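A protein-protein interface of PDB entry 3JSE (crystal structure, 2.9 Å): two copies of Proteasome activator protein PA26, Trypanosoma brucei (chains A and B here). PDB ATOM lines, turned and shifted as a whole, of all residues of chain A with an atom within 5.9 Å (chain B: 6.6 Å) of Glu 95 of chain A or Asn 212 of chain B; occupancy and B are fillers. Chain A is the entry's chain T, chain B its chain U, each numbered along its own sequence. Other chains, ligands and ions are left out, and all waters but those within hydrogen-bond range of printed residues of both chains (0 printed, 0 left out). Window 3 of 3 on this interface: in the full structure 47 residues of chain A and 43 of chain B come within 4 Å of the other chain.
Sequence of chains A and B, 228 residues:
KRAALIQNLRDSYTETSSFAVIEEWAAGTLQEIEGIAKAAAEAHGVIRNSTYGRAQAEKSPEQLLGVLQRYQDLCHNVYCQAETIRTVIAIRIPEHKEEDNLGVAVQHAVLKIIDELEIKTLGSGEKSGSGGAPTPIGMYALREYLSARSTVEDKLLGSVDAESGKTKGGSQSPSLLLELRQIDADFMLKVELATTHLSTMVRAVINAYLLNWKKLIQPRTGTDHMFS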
ATOM      1  N   ILE A  93       1.342  29.121 -15.639  1.00  0.00           N
ATOM      2  CA  ILE A  93       1.453  27.913 -16.450  1.00  0.00           C
ATOM      3  C   ILE A  93       0.370  26.974 -15.920  1.00  0.00           C
ATOM      4  O   ILE A  93       0.405  26.572 -14.747  1.00  0.00           O
ATOM      5  CB  ILE A  93       2.844  27.237 -16.338  1.00  0.00           C
ATOM      6  CG1 ILE A  93       3.898  28.081 -17.058  1.00  0.00           C
ATOM      7  CG2 ILE A  93       2.841  25.805 -16.892  1.00  0.00           C
ATOM      8  CD1 ILE A  93       5.323  27.726 -16.644  1.00  0.00           C
ATOM      9  N   PRO A  94      -0.599  26.616 -16.777  1.00  0.00           N
ATOM     10  CA  PRO A  94      -1.762  25.891 -16.334  1.00  0.00           C
ATOM     11  C   PRO A  94      -1.510  24.393 -16.164  1.00  0.00           C
ATOM     12  O   PRO A  94      -0.433  23.877 -16.504  1.00  0.00           O
ATOM     13  CB  PRO A  94      -2.746  26.139 -17.472  1.00  0.00           C
ATOM     14  CG  PRO A  94      -1.892  26.146 -18.686  1.00  0.00           C
ATOM     15  CD  PRO A  94      -0.562  26.718 -18.245  1.00  0.00           C
ATOM     16  N   GLU A  95      -2.543  23.716 -15.671  1.00  0.00           N
ATOM     17  CA  GLU A  95      -2.560  22.257 -15.525  1.00  0.00           C
ATOM     18  C   GLU A  95      -1.913  21.602 -16.736  1.00  0.00           C
ATOM     19  O   GLU A  95      -2.265  21.938 -17.856  1.00  0.00           O
ATOM     20  CB  GLU A  95      -4.012  21.792 -15.401  1.00  0.00           C
ATOM     21  CG  GLU A  95      -4.217  20.303 -15.241  1.00  0.00           C
ATOM     22  CD  GLU A  95      -5.695  19.938 -15.211  1.00  0.00           C
ATOM     23  OE1 GLU A  95      -6.414  20.551 -14.398  1.00  0.00           O
ATOM     24  OE2 GLU A  95      -6.135  19.045 -15.972  1.00  0.00           O
ATOM     25  N   HIS A  96      -0.994  20.669 -16.497  1.00  0.00           N
ATOM     26  CA  HIS A  96      -0.355  19.902 -17.543  1.00  0.00           C
ATOM     27  C   HIS A  96      -1.359  19.062 -18.282  1.00  0.00           C
ATOM     28  O   HIS A  96      -2.141  18.366 -17.660  1.00  0.00           O
ATOM     29  CB  HIS A  96       0.687  18.976 -16.962  1.00  0.00           C
ATOM     30  CG  HIS A  96       1.547  18.315 -18.001  1.00  0.00           C
ATOM     31  ND1 HIS A  96       2.743  18.849 -18.437  1.00  0.00           N
ATOM     32  CD2 HIS A  96       1.384  17.147 -18.678  1.00  0.00           C
ATOM     33  CE1 HIS A  96       3.273  18.037 -19.333  1.00  0.00           C
ATOM     34  NE2 HIS A  96       2.475  16.996 -19.496  1.00  0.00           N
ATOM     35  N   LYS A  97      -1.324  19.140 -19.613  1.00  0.00           N
ATOM     36  CA  LYS A  97      -2.216  18.389 -20.474  1.00  0.00           C
ATOM     37  C   LYS A  97      -1.484  18.109 -21.777  1.00  0.00           C
ATOM     38  O   LYS A  97      -0.511  18.794 -22.090  1.00  0.00           O
ATOM     39  CB  LYS A  97      -3.454  19.222 -20.786  1.00  0.00           C
ATOM     40  CG  LYS A  97      -4.374  19.468 -19.634  1.00  0.00           C
ATOM     41  CD  LYS A  97      -5.541  20.282 -20.109  1.00  0.00           C
ATOM     42  CE  LYS A  97      -6.598  20.398 -19.032  1.00  0.00           C
ATOM     43  NZ  LYS A  97      -7.413  19.195 -18.954  1.00  0.00           N
ATOM     44  N   ASN A 101      -2.398  23.467 -25.739  1.00  0.00           N
ATOM     45  CA  ASN A 101      -1.117  24.000 -25.288  1.00  0.00           C
ATOM     46  C   ASN A 101      -0.602  25.114 -26.200  1.00  0.00           C
ATOM     47  O   ASN A 101       0.578  25.403 -26.234  1.00  0.00           O
ATOM     48  CB  ASN A 101      -0.099  22.860 -25.175  1.00  0.00           C
ATOM     49  CG  ASN A 101      -0.415  21.905 -24.043  1.00  0.00           C
ATOM     50  OD1 ASN A 101      -0.785  22.325 -22.963  1.00  0.00           O
ATOM     51  ND2 ASN A 101      -0.276  20.619 -24.290  1.00  0.00           N
ATOM     52  N   ARG A 220      -5.181  29.739 -21.992  1.00  0.00           N
ATOM     53  CA  ARG A 220      -6.309  28.918 -22.397  1.00  0.00           C
ATOM     54  C   ARG A 220      -7.575  29.711 -22.152  1.00  0.00           C
ATOM     55  O   ARG A 220      -7.780  30.258 -21.060  1.00  0.00           O
ATOM     56  CB  ARG A 220      -6.369  27.633 -21.580  1.00  0.00           C
ATOM     57  CG  ARG A 220      -5.272  26.655 -21.876  1.00  0.00           C
ATOM     58  CD  ARG A 220      -5.385  25.440 -21.017  1.00  0.00           C
ATOM     59  NE  ARG A 220      -4.301  24.526 -21.299  1.00  0.00           N
ATOM     60  CZ  ARG A 220      -3.846  23.607 -20.456  1.00  0.00           C
ATOM     61  NH1 ARG A 220      -4.386  23.466 -19.255  1.00  0.00           N
ATOM     62  NH2 ARG A 220      -2.845  22.810 -20.816  1.00  0.00           N
ATOM     63  N   VAL B 106       2.077  13.982 -16.116  1.00  0.00           N
ATOM     64  CA  VAL B 106       1.984  15.008 -15.056  1.00  0.00           C
ATOM     65  C   VAL B 106       2.964  14.723 -13.895  1.00  0.00           C
ATOM     66  O   VAL B 106       3.695  15.605 -13.441  1.00  0.00           O
ATOM     67  CB  VAL B 106       0.550  15.089 -14.456  1.00  0.00           C
ATOM     68  CG1 VAL B 106       0.492  16.047 -13.249  1.00  0.00           C
ATOM     69  CG2 VAL B 106      -0.437  15.518 -15.510  1.00  0.00           C
ATOM     70  N   VAL B 110       6.071  17.286 -13.021  1.00  0.00           N
ATOM     71  CA  VAL B 110       6.240  17.969 -11.737  1.00  0.00           C
ATOM     72  C   VAL B 110       7.522  17.543 -11.037  1.00  0.00           C
ATOM     73  O   VAL B 110       8.178  18.342 -10.399  1.00  0.00           O
ATOM     74  CB  VAL B 110       5.030  17.781 -10.806  1.00  0.00           C
ATOM     75  CG1 VAL B 110       5.333  18.270  -9.434  1.00  0.00           C
ATOM     76  CG2 VAL B 110       3.857  18.531 -11.355  1.00  0.00           C
ATOM     77  N   ASN B 207       2.431  26.761  -7.671  1.00  0.00           N
ATOM     78  CA  ASN B 207       1.430  26.709  -8.736  1.00  0.00           C
ATOM     79  C   ASN B 207       1.344  25.329  -9.456  1.00  0.00           C
ATOM     80  O   ASN B 207       0.269  24.738  -9.558  1.00  0.00           O
ATOM     81  CB  ASN B 207       1.728  27.841  -9.711  1.00  0.00           C
ATOM     82  CG  ASN B 207       0.818  27.856 -10.845  1.00  0.00           C
ATOM     83  OD1 ASN B 207      -0.382  28.082 -10.679  1.00  0.00           O
ATOM     84  ND2 ASN B 207       1.362  27.623 -12.030  1.00  0.00           N
ATOM     85  N   ALA B 208       2.484  24.813  -9.920  1.00  0.00           N
ATOM     86  CA  ALA B 208       2.545  23.515 -10.570  1.00  0.00           C
ATOM     87  C   ALA B 208       1.904  22.445  -9.697  1.00  0.00           C
ATOM     88  O   ALA B 208       1.151  21.617 -10.200  1.00  0.00           O
ATOM     89  CB  ALA B 208       3.969  23.145 -10.932  1.00  0.00           C
ATOM     90  N   TYR B 209       2.163  22.472  -8.389  1.00  0.00           N
ATOM     91  CA  TYR B 209       1.542  21.477  -7.481  1.00  0.00           C
ATOM     92  C   TYR B 209       0.035  21.650  -7.339  1.00  0.00           C
ATOM     93  O   TYR B 209      -0.699  20.692  -7.496  1.00  0.00           O
ATOM     94  CB  TYR B 209       2.133  21.501  -6.079  1.00  0.00           C
ATOM     95  CG  TYR B 209       1.597  20.406  -5.171  1.00  0.00           C
ATOM     96  CD1 TYR B 209       2.230  19.167  -5.107  1.00  0.00           C
ATOM     97  CD2 TYR B 209       0.478  20.613  -4.367  1.00  0.00           C
ATOM     98  CE1 TYR B 209       1.774  18.166  -4.274  1.00  0.00           C
ATOM     99  CE2 TYR B 209      -0.010  19.605  -3.524  1.00  0.00           C
ATOM    100  CZ  TYR B 209       0.638  18.376  -3.476  1.00  0.00           C
ATOM    101  OH  TYR B 209       0.190  17.348  -2.649  1.00  0.00           O
ATOM    102  N   LEU B 210      -0.426  22.840  -7.006  1.00  0.00           N
ATOM    103  CA  LEU B 210      -1.835  22.980  -6.715  1.00  0.00           C
ATOM    104  C   LEU B 210      -2.729  22.738  -7.960  1.00  0.00           C
ATOM    105  O   LEU B 210      -3.867  22.208  -7.836  1.00  0.00           O
ATOM    106  CB  LEU B 210      -2.128  24.323  -6.071  1.00  0.00           C
ATOM    107  CG  LEU B 210      -1.534  24.496  -4.670  1.00  0.00           C
ATOM    108  CD1 LEU B 210      -1.806  25.904  -4.171  1.00  0.00           C
ATOM    109  CD2 LEU B 210      -2.078  23.455  -3.715  1.00  0.00           C
ATOM    110  N   LEU B 211      -2.231  23.078  -9.154  1.00  0.00           N
ATOM    111  CA  LEU B 211      -2.969  22.755 -10.383  1.00  0.00           C
ATOM    112  C   LEU B 211      -2.982  21.254 -10.704  1.00  0.00           C
ATOM    113  O   LEU B 211      -3.897  20.802 -11.341  1.00  0.00           O
ATOM    114  CB  LEU B 211      -2.429  23.538 -11.589  1.00  0.00           C
ATOM    115  CG  LEU B 211      -2.574  25.070 -11.590  1.00  0.00           C
ATOM    116  CD1 LEU B 211      -1.881  25.672 -12.805  1.00  0.00           C
ATOM    117  CD2 LEU B 211      -4.040  25.513 -11.505  1.00  0.00           C
ATOM    118  N   ASN B 212      -2.004  20.480 -10.262  1.00  0.00           N
ATOM    119  CA  ASN B 212      -1.856  19.114 -10.753  1.00  0.00           C
ATOM    120  C   ASN B 212      -1.977  18.009  -9.702  1.00  0.00           C
ATOM    121  O   ASN B 212      -1.668  16.843  -9.958  1.00  0.00           O
ATOM    122  CB  ASN B 212      -0.502  18.989 -11.489  1.00  0.00           C
ATOM    123  CG  ASN B 212      -0.461  19.820 -12.756  1.00  0.00           C
ATOM    124  OD1 ASN B 212      -1.219  19.573 -13.667  1.00  0.00           O
ATOM    125  ND2 ASN B 212       0.387  20.820 -12.802  1.00  0.00           N
ATOM    126  N   TRP B 213      -2.432  18.353  -8.513  1.00  0.00           N
ATOM    127  CA  TRP B 213      -2.214  17.442  -7.399  1.00  0.00           C
ATOM    128  C   TRP B 213      -3.022  16.183  -7.492  1.00  0.00           C
ATOM    129  O   TRP B 213      -2.618  15.148  -6.992  1.00  0.00           O
ATOM    130  CB  TRP B 213      -2.471  18.131  -6.066  1.00  0.00           C
ATOM    131  CG  TRP B 213      -3.872  18.446  -5.784  1.00  0.00           C
ATOM    132  CD1 TRP B 213      -4.499  19.601  -6.056  1.00  0.00           C
ATOM    133  CD2 TRP B 213      -4.826  17.609  -5.117  1.00  0.00           C
ATOM    134  NE1 TRP B 213      -5.798  19.545  -5.614  1.00  0.00           N
ATOM    135  CE2 TRP B 213      -6.021  18.324  -5.041  1.00  0.00           C
ATOM    136  CE3 TRP B 213      -4.790  16.310  -4.604  1.00  0.00           C
ATOM    137  CZ2 TRP B 213      -7.172  17.789  -4.476  1.00  0.00           C
ATOM    138  CZ3 TRP B 213      -5.952  15.771  -4.042  1.00  0.00           C
ATOM    139  CH2 TRP B 213      -7.112  16.510  -3.980  1.00  0.00           C
ATOM    140  N   LYS B 214      -4.172  16.264  -8.134  1.00  0.00           N
ATOM    141  CA  LYS B 214      -5.048  15.096  -8.245  1.00  0.00           C
ATOM    142  C   LYS B 214      -4.442  13.988  -9.088  1.00  0.00           C
ATOM    143  O   LYS B 214      -4.474  12.827  -8.690  1.00  0.00           O
ATOM    144  CB  LYS B 214      -6.403  15.492  -8.809  1.00  0.00           C
ATOM    145  CG  LYS B 214      -7.300  16.096  -7.774  1.00  0.00           C
ATOM    146  CD  LYS B 214      -8.672  16.336  -8.328  1.00  0.00           C
ATOM    147  CE  LYS B 214      -9.413  17.391  -7.514  1.00  0.00           C
ATOM    148  NZ  LYS B 214     -10.307  18.221  -8.393  1.00  0.00           N
ATOM    149  N   LYS B 215      -3.891  14.350 -10.246  1.00  0.00           N
ATOM    150  CA  LYS B 215      -3.210  13.377 -11.085  1.00  0.00           C
ATOM    151  C   LYS B 215      -1.861  12.925 -10.511  1.00  0.00           C
ATOM    152  O   LYS B 215      -1.382  11.847 -10.867  1.00  0.00           O
ATOM    153  CB  LYS B 215      -3.024  13.908 -12.500  1.00  0.00           C
ATOM    154  CG  LYS B 215      -4.314  13.935 -13.350  1.00  0.00           C
ATOM    155  CD  LYS B 215      -4.771  12.544 -13.745  1.00  0.00           C
ATOM    156  CE  LYS B 215      -5.340  12.487 -15.178  1.00  0.00           C
ATOM    157  NZ  LYS B 215      -6.432  13.451 -15.351  1.00  0.00           N
ATOM    158  N   LEU B 216      -1.251  13.727  -9.625  1.00  0.00           N
ATOM    159  CA  LEU B 216      -0.025  13.297  -8.884  1.00  0.00           C
ATOM    160  C   LEU B 216      -0.294  12.122  -7.926  1.00  0.00           C
ATOM    161  O   LEU B 216       0.513  11.203  -7.812  1.00  0.00           O
ATOM    162  CB  LEU B 216       0.612  14.463  -8.144  1.00  0.00           C
ATOM    163  CG  LEU B 216       1.166  15.605  -9.012  1.00  0.00           C
ATOM    164  CD1 LEU B 216       1.848  16.666  -8.120  1.00  0.00           C
ATOM    165  CD2 LEU B 216       2.108  15.138 -10.117  1.00  0.00           C
ATOM    166  N   ILE B 217      -1.463  12.127  -7.284  1.00  0.00           N
ATOM    167  CA  ILE B 217      -1.862  11.038  -6.373  1.00  0.00           C
ATOM    168  C   ILE B 217      -2.524   9.846  -7.118  1.00  0.00           C
ATOM    169  O   ILE B 217      -2.114   8.720  -6.926  1.00  0.00           O
ATOM    170  CB  ILE B 217      -2.803  11.553  -5.246  1.00  0.00           C
ATOM    171  CG1 ILE B 217      -2.211  12.769  -4.571  1.00  0.00           C
ATOM    172  CG2 ILE B 217      -3.062  10.471  -4.252  1.00  0.00           C
ATOM    173  CD1 ILE B 217      -0.826  12.536  -4.083  1.00  0.00           C
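The backbone carbonyl oxygen (O) of Ile 93 of chain A lies within hydrogen-bond range of the side-chain amide nitrogen (ND2) of Asn 207 of chain B (3.1 Å).
The backbone NH (N) of His 96 of chain A is in hydrogen-bond range of the side-chain amide oxygen (OD1) of Asn 212 of chain B, 3.0 Å away.
OE2 of Glu 95 of chain A lies within salt-bridge range of NZ of Lys 97 of chain A.
O of Glu 95 of chain A is in hydrogen-bond range of NH1 of Arg 220 of chain A (3.0 Å).
O of Ala 208 of chain B is in hydrogen-bond range of ND2 of Asn 212 of chain B, 2.8 Å away.
Leu 211 of chain B touches Ile 93 of chain A (CD1 to O, 3.1 Å).
CD1 of Leu 211 of chain B touches CA of Pro 94 of chain A, 3.5 Å away.
Glu 95 of chain A touches Leu 211 of chain B.
CG of Glu 95 of chain A touches OD1 of Asn 212 of chain B, at 3.5 Å.
CB of His 96 of chain A touches CG2 of Val 106 of chain B, at 3.9 Å.
Glu 95 of chain A touches just these residues of chain B: Leu 211 and Asn 212.
Asn 212 of chain B touches just these residues of chain A: Glu 95 (3.5 Å) and His 96 (3.0 Å).
Printed residues of chain A within 4 Å of Asn 207 of chain B: Ile 93 (3.1 Å).
Printed residues of chain B within 4 Å of His 96 of chain A: Val 106 (3.9 Å) and Asn 212 (3.0 Å).
Of the printed residues of chain B, Pro 94 of chain A touches Leu 211 (3.5 Å).
Printed residues of chain A within 4 Å of Val 106 of chain B: His 96 (3.9 Å).
Leu 216 of chain B touches none of the printed residues of chain A.
The nearest residue of chain B that does not touch Glu 95 of chain A is Lys 215 of chain B (5.6 Å).
The nearest residue of chain A that does not touch Asn 212 of chain B is Pro 94 of chain A (4.9 Å).
Printed residues of chain A that touch a printed residue of chain B: Ile 93, Pro 94, Glu 95 and His 96.
Hydrophobic or aromatic side chains of chain A that line the printed part of chain B: His 96.
Along chain A the printed residues that touch a printed residue of chain B span positions 93 to 96.
Hydrophobic or aromatic side chains of chain B within 4 Å of the printed part of chain A: Val 106 and Leu 211.
No position is printed for both chains.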
